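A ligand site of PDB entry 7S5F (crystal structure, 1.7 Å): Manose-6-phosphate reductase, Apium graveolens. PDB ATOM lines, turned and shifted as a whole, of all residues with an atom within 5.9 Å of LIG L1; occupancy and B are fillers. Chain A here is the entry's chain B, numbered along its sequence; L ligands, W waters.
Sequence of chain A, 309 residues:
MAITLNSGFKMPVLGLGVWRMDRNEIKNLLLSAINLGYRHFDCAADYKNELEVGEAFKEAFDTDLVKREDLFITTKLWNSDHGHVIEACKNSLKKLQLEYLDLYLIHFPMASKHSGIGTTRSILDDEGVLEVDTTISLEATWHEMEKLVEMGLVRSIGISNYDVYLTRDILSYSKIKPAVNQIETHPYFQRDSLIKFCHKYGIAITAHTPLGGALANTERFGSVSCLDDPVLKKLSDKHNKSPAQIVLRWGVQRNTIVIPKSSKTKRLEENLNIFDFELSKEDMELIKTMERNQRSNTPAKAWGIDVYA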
ATOM      1  N   TRP A  19     -27.991  15.227   7.442  1.00  0.00           N
ATOM      2  CA  TRP A  19     -28.279  14.747   8.789  1.00  0.00           C
ATOM      3  C   TRP A  19     -29.781  14.852   9.066  1.00  0.00           C
ATOM      4  O   TRP A  19     -30.413  15.851   8.725  1.00  0.00           O
ATOM      5  CB  TRP A  19     -27.481  15.550   9.828  1.00  0.00           C
ATOM      6  CG  TRP A  19     -27.719  15.078  11.223  1.00  0.00           C
ATOM      7  CD1 TRP A  19     -27.796  13.781  11.666  1.00  0.00           C
ATOM      8  CD2 TRP A  19     -27.939  15.899  12.381  1.00  0.00           C
ATOM      9  NE1 TRP A  19     -28.042  13.748  13.015  1.00  0.00           N
ATOM     10  CE2 TRP A  19     -28.133  15.034  13.479  1.00  0.00           C
ATOM     11  CE3 TRP A  19     -27.984  17.291  12.581  1.00  0.00           C
ATOM     12  CZ2 TRP A  19     -28.378  15.512  14.765  1.00  0.00           C
ATOM     13  CZ3 TRP A  19     -28.214  17.757  13.857  1.00  0.00           C
ATOM     14  CH2 TRP A  19     -28.411  16.875  14.941  1.00  0.00           C
ATOM     15  N   ALA A  44     -22.074  12.035   6.359  1.00  0.00           N
ATOM     16  CA  ALA A  44     -21.212  11.541   7.423  1.00  0.00           C
ATOM     17  C   ALA A  44     -21.517  10.059   7.600  1.00  0.00           C
ATOM     18  O   ALA A  44     -22.665   9.637   7.446  1.00  0.00           O
ATOM     19  CB  ALA A  44     -21.414  12.274   8.743  1.00  0.00           C
ATOM     20  N   ASP A  46     -21.692   8.596  10.398  1.00  0.00           N
ATOM     21  CA  ASP A  46     -22.557   8.471  11.554  1.00  0.00           C
ATOM     22  C   ASP A  46     -23.968   9.017  11.327  1.00  0.00           C
ATOM     23  O   ASP A  46     -24.782   8.945  12.253  1.00  0.00           O
ATOM     24  CB  ASP A  46     -21.919   9.175  12.755  1.00  0.00           C
ATOM     25  CG  ASP A  46     -22.403   8.622  14.065  1.00  0.00           C
ATOM     26  OD1 ASP A  46     -22.437   7.383  14.216  1.00  0.00           O
ATOM     27  OD2 ASP A  46     -22.756   9.433  14.949  1.00  0.00           O
ATOM     28  N   TYR A  47     -24.275   9.554  10.151  1.00  0.00           N
ATOM     29  CA  TYR A  47     -25.665   9.878   9.854  1.00  0.00           C
ATOM     30  C   TYR A  47     -26.448   8.644   9.446  1.00  0.00           C
ATOM     31  O   TYR A  47     -27.680   8.718   9.333  1.00  0.00           O
ATOM     32  CB  TYR A  47     -25.759  10.931   8.739  1.00  0.00           C
ATOM     33  CG  TYR A  47     -25.082  12.260   9.042  1.00  0.00           C
ATOM     34  CD1 TYR A  47     -24.714  12.605  10.342  1.00  0.00           C
ATOM     35  CD2 TYR A  47     -24.782  13.143   8.013  1.00  0.00           C
ATOM     36  CE1 TYR A  47     -24.080  13.804  10.612  1.00  0.00           C
ATOM     37  CE2 TYR A  47     -24.145  14.341   8.269  1.00  0.00           C
ATOM     38  CZ  TYR A  47     -23.802  14.665   9.563  1.00  0.00           C
ATOM     39  OH  TYR A  47     -23.158  15.855   9.800  1.00  0.00           O
ATOM     40  N   LYS A  48     -25.768   7.515   9.230  1.00  0.00           N
ATOM     41  CA  LYS A  48     -26.364   6.194   9.026  1.00  0.00           C
ATOM     42  C   LYS A  48     -27.154   6.093   7.719  1.00  0.00           C
ATOM     43  O   LYS A  48     -28.009   5.216   7.589  1.00  0.00           O
ATOM     44  CB  LYS A  48     -27.257   5.788  10.204  1.00  0.00           C
ATOM     45  CG  LYS A  48     -26.554   5.845  11.565  1.00  0.00           C
ATOM     46  CD  LYS A  48     -25.264   5.034  11.564  1.00  0.00           C
ATOM     47  CE  LYS A  48     -24.573   5.072  12.908  1.00  0.00           C
ATOM     48  NZ  LYS A  48     -25.295   4.289  13.952  1.00  0.00           N
ATOM     49  N   LYS A  76     -17.432  12.050   6.600  1.00  0.00           N
ATOM     50  CA  LYS A  76     -16.714  12.336   7.829  1.00  0.00           C
ATOM     51  C   LYS A  76     -16.360  11.056   8.582  1.00  0.00           C
ATOM     52  O   LYS A  76     -17.117  10.078   8.591  1.00  0.00           O
ATOM     53  CB  LYS A  76     -17.527  13.250   8.754  1.00  0.00           C
ATOM     54  CG  LYS A  76     -18.154  14.442   8.039  1.00  0.00           C
ATOM     55  CD  LYS A  76     -18.756  15.432   9.020  1.00  0.00           C
ATOM     56  CE  LYS A  76     -19.559  16.508   8.282  1.00  0.00           C
ATOM     57  NZ  LYS A  76     -20.868  15.984   7.802  1.00  0.00           N
ATOM     58  N   TRP A  78     -16.072   9.129  11.899  1.00  0.00           N
ATOM     59  CA  TRP A  78     -16.700   9.222  13.205  1.00  0.00           C
ATOM     60  C   TRP A  78     -15.675   9.035  14.323  1.00  0.00           C
ATOM     61  O   TRP A  78     -14.592   8.455  14.134  1.00  0.00           O
ATOM     62  CB  TRP A  78     -17.832   8.191  13.385  1.00  0.00           C
ATOM     63  CG  TRP A  78     -18.570   8.452  14.662  1.00  0.00           C
ATOM     64  CD1 TRP A  78     -18.738   7.603  15.722  1.00  0.00           C
ATOM     65  CD2 TRP A  78     -19.194   9.701  15.047  1.00  0.00           C
ATOM     66  NE1 TRP A  78     -19.426   8.234  16.737  1.00  0.00           N
ATOM     67  CE2 TRP A  78     -19.716   9.518  16.342  1.00  0.00           C
ATOM     68  CE3 TRP A  78     -19.354  10.944  14.410  1.00  0.00           C
ATOM     69  CZ2 TRP A  78     -20.411  10.533  17.014  1.00  0.00           C
ATOM     70  CZ3 TRP A  78     -20.036  11.954  15.077  1.00  0.00           C
ATOM     71  CH2 TRP A  78     -20.552  11.744  16.375  1.00  0.00           C
ATOM     72  N   HIS A 107     -14.754  14.240  12.178  1.00  0.00           N
ATOM     73  CA  HIS A 107     -16.090  14.737  12.542  1.00  0.00           C
ATOM     74  C   HIS A 107     -16.046  15.574  13.823  1.00  0.00           C
ATOM     75  O   HIS A 107     -16.695  16.629  13.898  1.00  0.00           O
ATOM     76  CB  HIS A 107     -17.051  13.553  12.701  1.00  0.00           C
ATOM     77  CG  HIS A 107     -18.501  13.907  12.533  1.00  0.00           C
ATOM     78  ND1 HIS A 107     -19.398  13.055  11.924  1.00  0.00           N
ATOM     79  CD2 HIS A 107     -19.210  14.996  12.913  1.00  0.00           C
ATOM     80  CE1 HIS A 107     -20.602  13.615  11.924  1.00  0.00           C
ATOM     81  NE2 HIS A 107     -20.505  14.791  12.521  1.00  0.00           N
ATOM     82  N   PHE A 108     -15.316  15.109  14.831  1.00  0.00           N
ATOM     83  CA  PHE A 108     -15.148  15.806  16.099  1.00  0.00           C
ATOM     84  C   PHE A 108     -13.713  15.613  16.560  1.00  0.00           C
ATOM     85  O   PHE A 108     -13.094  14.599  16.257  1.00  0.00           O
ATOM     86  CB  PHE A 108     -16.067  15.247  17.198  1.00  0.00           C
ATOM     87  CG  PHE A 108     -17.478  15.754  17.149  1.00  0.00           C
ATOM     88  CD1 PHE A 108     -17.851  16.916  17.820  1.00  0.00           C
ATOM     89  CD2 PHE A 108     -18.457  15.036  16.469  1.00  0.00           C
ATOM     90  CE1 PHE A 108     -19.155  17.362  17.786  1.00  0.00           C
ATOM     91  CE2 PHE A 108     -19.761  15.475  16.443  1.00  0.00           C
ATOM     92  CZ  PHE A 108     -20.111  16.649  17.097  1.00  0.00           C
ATOM     93  N   GLN A 182     -15.306  22.646   9.457  1.00  0.00           N
ATOM     94  CA  GLN A 182     -16.760  22.729   9.426  1.00  0.00           C
ATOM     95  C   GLN A 182     -17.254  22.932  10.854  1.00  0.00           C
ATOM     96  O   GLN A 182     -17.127  22.046  11.691  1.00  0.00           O
ATOM     97  CB  GLN A 182     -17.394  21.477   8.809  1.00  0.00           C
ATOM     98  CG  GLN A 182     -18.918  21.474   8.941  1.00  0.00           C
ATOM     99  CD  GLN A 182     -19.583  20.273   8.313  1.00  0.00           C
ATOM    100  OE1 GLN A 182     -20.434  19.633   8.937  1.00  0.00           O
ATOM    101  NE2 GLN A 182     -19.222  19.964   7.069  1.00  0.00           N
ATOM    102  N   ARG A 220     -34.783  19.407  19.673  1.00  0.00           N
ATOM    103  CA  ARG A 220     -33.728  18.466  20.043  1.00  0.00           C
ATOM    104  C   ARG A 220     -32.764  19.050  21.069  1.00  0.00           C
ATOM    105  O   ARG A 220     -32.303  18.336  21.966  1.00  0.00           O
ATOM    106  CB  ARG A 220     -32.961  18.025  18.798  1.00  0.00           C
ATOM    107  CG  ARG A 220     -31.818  17.066  19.088  1.00  0.00           C
ATOM    108  CD  ARG A 220     -31.014  16.728  17.840  1.00  0.00           C
ATOM    109  NE  ARG A 220     -31.532  15.579  17.114  1.00  0.00           N
ATOM    110  CZ  ARG A 220     -31.160  14.333  17.345  1.00  0.00           C
ATOM    111  NH1 ARG A 220     -30.235  14.034  18.247  1.00  0.00           N
ATOM    112  NH2 ARG A 220     -31.713  13.353  16.631  1.00  0.00           N
ATOM    113  N   PHE A 221     -32.446  20.339  20.964  1.00  0.00           N
ATOM    114  CA  PHE A 221     -31.438  20.964  21.802  1.00  0.00           C
ATOM    115  C   PHE A 221     -31.957  22.087  22.687  1.00  0.00           C
ATOM    116  O   PHE A 221     -31.244  22.527  23.586  1.00  0.00           O
ATOM    117  CB  PHE A 221     -30.289  21.523  20.943  1.00  0.00           C
ATOM    118  CG  PHE A 221     -29.591  20.489  20.098  1.00  0.00           C
ATOM    119  CD1 PHE A 221     -28.862  19.467  20.683  1.00  0.00           C
ATOM    120  CD2 PHE A 221     -29.627  20.577  18.713  1.00  0.00           C
ATOM    121  CE1 PHE A 221     -28.200  18.526  19.890  1.00  0.00           C
ATOM    122  CE2 PHE A 221     -28.978  19.641  17.924  1.00  0.00           C
ATOM    123  CZ  PHE A 221     -28.261  18.617  18.520  1.00  0.00           C
ATOM    124  N   ASN A 297     -26.258  23.335  18.567  1.00  0.00           N
ATOM    125  CA  ASN A 297     -25.999  21.905  18.495  1.00  0.00           C
ATOM    126  C   ASN A 297     -24.916  21.545  19.505  1.00  0.00           C
ATOM    127  O   ASN A 297     -23.803  22.051  19.442  1.00  0.00           O
ATOM    128  CB  ASN A 297     -25.527  21.524  17.085  1.00  0.00           C
ATOM    129  CG  ASN A 297     -25.346  20.035  16.909  1.00  0.00           C
ATOM    130  OD1 ASN A 297     -24.531  19.403  17.605  1.00  0.00           O
ATOM    131  ND2 ASN A 297     -26.000  19.473  15.893  1.00  0.00           N
ATOM    132  N   PRO A 299     -23.442  17.795  21.535  1.00  0.00           N
ATOM    133  CA  PRO A 299     -23.587  16.359  21.792  1.00  0.00           C
ATOM    134  C   PRO A 299     -23.603  15.977  23.267  1.00  0.00           C
ATOM    135  O   PRO A 299     -23.488  14.790  23.584  1.00  0.00           O
ATOM    136  CB  PRO A 299     -22.328  15.782  21.122  1.00  0.00           C
ATOM    137  CG  PRO A 299     -21.288  16.837  21.354  1.00  0.00           C
ATOM    138  CD  PRO A 299     -22.040  18.173  21.287  1.00  0.00           C
ATOM    139  N   TRP A 303     -23.594  12.077  24.619  1.00  0.00           N
ATOM    140  CA  TRP A 303     -22.365  11.514  25.144  1.00  0.00           C
ATOM    141  C   TRP A 303     -22.316  11.496  26.667  1.00  0.00           C
ATOM    142  O   TRP A 303     -21.426  10.859  27.228  1.00  0.00           O
ATOM    143  CB  TRP A 303     -21.146  12.279  24.619  1.00  0.00           C
ATOM    144  CG  TRP A 303     -21.050  12.320  23.131  1.00  0.00           C
ATOM    145  CD1 TRP A 303     -21.769  11.573  22.232  1.00  0.00           C
ATOM    146  CD2 TRP A 303     -20.166  13.133  22.352  1.00  0.00           C
ATOM    147  NE1 TRP A 303     -21.402  11.896  20.949  1.00  0.00           N
ATOM    148  CE2 TRP A 303     -20.419  12.845  20.998  1.00  0.00           C
ATOM    149  CE3 TRP A 303     -19.194  14.087  22.668  1.00  0.00           C
ATOM    150  CZ2 TRP A 303     -19.732  13.474  19.954  1.00  0.00           C
ATOM    151  CZ3 TRP A 303     -18.519  14.713  21.636  1.00  0.00           C
ATOM    152  CH2 TRP A 303     -18.783  14.410  20.295  1.00  0.00           C
HETATM  153  C1  LIG L   1     -23.911  16.210  14.416  1.00  0.00           C
HETATM  154  C2  LIG L   1     -23.611  14.816  14.980  1.00  0.00           C
HETATM  155  O1  LIG L   1     -24.940  16.512  12.292  1.00  0.00           O
HETATM  156  C3  LIG L   1     -23.882  16.228  12.920  1.00  0.00           C
HETATM  157  O2  LIG L   1     -22.789  16.002  12.350  1.00  0.00           O
HETATM  158  O3  LIG L   1     -25.214  16.628  14.859  1.00  0.00           O
HETATM  159  O4  LIG L   1     -23.383  14.944  16.394  1.00  0.00           O
HETATM  160  C4  LIG L   1     -24.813  13.897  14.795  1.00  0.00           C
HETATM  161  O5  LIG L   1     -25.802  14.269  15.755  1.00  0.00           O
HETATM  162  C5  LIG L   1     -24.462  12.429  15.046  1.00  0.00           C
HETATM  163  O6  LIG L   1     -23.367  12.022  14.216  1.00  0.00           O
HETATM  164  C6  LIG L   1     -25.681  11.558  14.745  1.00  0.00           C
HETATM  165  O7  LIG L   1     -25.428  10.202  15.156  1.00  0.00           O
HETATM  166  P1  LG2 L   2     -29.928  23.704   9.676  1.00  0.00           P
HETATM  167  O1  LG2 L   2     -29.387  24.996  10.195  1.00  0.00           O
HETATM  168  O2  LG2 L   2     -29.566  23.397   8.249  1.00  0.00           O
HETATM  169  O3  LG2 L   2     -31.527  23.795   9.755  1.00  0.00           O
HETATM  170  C1  LG2 L   2     -32.299  22.620   9.464  1.00  0.00           C
HETATM  171  C2  LG2 L   2     -33.734  22.880   9.874  1.00  0.00           C
HETATM  172  O4  LG2 L   2     -34.222  24.042   9.189  1.00  0.00           O
HETATM  173  C3  LG2 L   2     -34.637  21.736   9.476  1.00  0.00           C
HETATM  174  O5  LG2 L   2     -35.535  21.485  10.550  1.00  0.00           O
HETATM  175  C4  LG2 L   2     -35.405  22.236   8.274  1.00  0.00           C
HETATM  176  O6  LG2 L   2     -36.729  21.714   8.307  1.00  0.00           O
HETATM  177  C5  LG2 L   2     -35.420  23.739   8.491  1.00  0.00           C
HETATM  178  N1  LG2 L   2     -35.396  24.487   7.210  1.00  0.00           N
HETATM  179  C6  LG2 L   2     -34.604  24.239   6.143  1.00  0.00           C
HETATM  180  N2  LG2 L   2     -34.821  25.147   5.166  1.00  0.00           N
HETATM  181  C7  LG2 L   2     -35.767  25.991   5.609  1.00  0.00           C
HETATM  182  C8  LG2 L   2     -36.470  27.186   5.080  1.00  0.00           C
HETATM  183  N3  LG2 L   2     -36.196  27.662   3.846  1.00  0.00           N
HETATM  184  N4  LG2 L   2     -37.384  27.778   5.887  1.00  0.00           N
HETATM  185  C9  LG2 L   2     -37.664  27.324   7.125  1.00  0.00           C
HETATM  186  N5  LG2 L   2     -37.076  26.235   7.664  1.00  0.00           N
HETATM  187  C10 LG2 L   2     -36.132  25.552   6.964  1.00  0.00           C
HETATM  188  O7  LG2 L   2     -29.500  22.537  10.711  1.00  0.00           O
HETATM  189  P2  LG2 L   2     -28.712  21.173  10.388  1.00  0.00           P
HETATM  190  O8  LG2 L   2     -28.503  20.476  11.702  1.00  0.00           O
HETATM  191  O9  LG2 L   2     -29.480  20.318   9.410  1.00  0.00           O
HETATM  192  O10 LG2 L   2     -27.282  21.525   9.776  1.00  0.00           O
HETATM  193  C11 LG2 L   2     -27.115  21.467   8.362  1.00  0.00           C
HETATM  194  C12 LG2 L   2     -26.194  20.326   7.994  1.00  0.00           C
HETATM  195  O11 LG2 L   2     -24.905  20.543   8.580  1.00  0.00           O
HETATM  196  C13 LG2 L   2     -26.635  18.957   8.488  1.00  0.00           C
HETATM  197  O12 LG2 L   2     -27.631  18.344   7.674  1.00  0.00           O
HETATM  198  C14 LG2 L   2     -25.321  18.210   8.489  1.00  0.00           C
HETATM  199  O13 LG2 L   2     -25.052  17.831   7.132  1.00  0.00           O
HETATM  200  C15 LG2 L   2     -24.310  19.274   8.926  1.00  0.00           C
HETATM  201  N6  LG2 L   2     -24.019  19.295  10.369  1.00  0.00           N
HETATM  202  C16 LG2 L   2     -22.789  18.954  10.780  1.00  0.00           C
HETATM  203  C17 LG2 L   2     -22.459  18.983  12.137  1.00  0.00           C
HETATM  204  C18 LG2 L   2     -21.080  18.607  12.587  1.00  0.00           C
HETATM  205  O14 LG2 L   2     -20.911  18.346  13.774  1.00  0.00           O
HETATM  206  N7  LG2 L   2     -20.091  18.622  11.695  1.00  0.00           N
HETATM  207  C19 LG2 L   2     -23.394  19.360  13.089  1.00  0.00           C
HETATM  208  C20 LG2 L   2     -24.673  19.737  12.708  1.00  0.00           C
HETATM  209  C21 LG2 L   2     -25.065  19.740  11.311  1.00  0.00           C
HETATM  210  P3  LG2 L   2     -37.278  20.764   7.133  1.00  0.00           P
HETATM  211  O15 LG2 L   2     -38.603  20.192   7.585  1.00  0.00           O
HETATM  212  O16 LG2 L   2     -37.417  21.610   5.895  1.00  0.00           O
HETATM  213  O17 LG2 L   2     -36.303  19.627   6.888  1.00  0.00           O
HETATM  214  O   HOH W   1     -24.613  16.799  18.195  1.00  0.00           O
HETATM  215  O   HOH W   2     -25.793  12.986  18.473  1.00  0.00           O
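The side-chain hydroxyl of Tyr 47 is in hydrogen-bond range of the side-chain amino group of Lys 76 (3.0 Å).
The side-chain amide nitrogen of Asn 297 sits at hydrogen-bond distance from an oxygen (O3) of LIG L1 (3.1 Å).
A ring nitrogen (NE2) of His 107 is in hydrogen-bond range of an oxygen (O2) of LIG L1 (2.6 Å).
N7 of LG2 L2 sits at hydrogen-bond distance from OE1 of Gln 182 (3.0 Å).
O2 of LIG L1 lies within hydrogen-bond range of OH of Tyr 47 (2.6 Å).
The backbone carbonyl oxygen (O) of Asp 46 is in hydrogen-bond range of an oxygen (O7) of LIG L1, at 3.2 Å.
O12 of LG2 L2 sits at hydrogen-bond distance from N of Trp 19 (3.1 Å).
An oxygen (O6) of LIG L1 lies within hydrogen-bond range of the side-chain carboxylate (OD2) of Asp 46, at 2.8 Å.
CZ2 of Trp 19 touches O5 of LIG L1, at 3.0 Å.
Trp 78 touches LIG L1.
CE2 of Phe 108 touches O4 of LIG L1, 3.7 Å away.
Hydrophobic or aromatic side chains that line LIG L1: Trp 19, Tyr 47, Trp 78, His 107 and Phe 108.
Of the 15 residues printed, 7 come within 4 Å of LIG L1.
The nearest printed residue that does not touch LIG L1 is Pro 299 (4.9 Å).
Water W1 bridges OD1 of Asn 297 (2.7 Å) and O4 of LIG L1 (2.9 Å).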
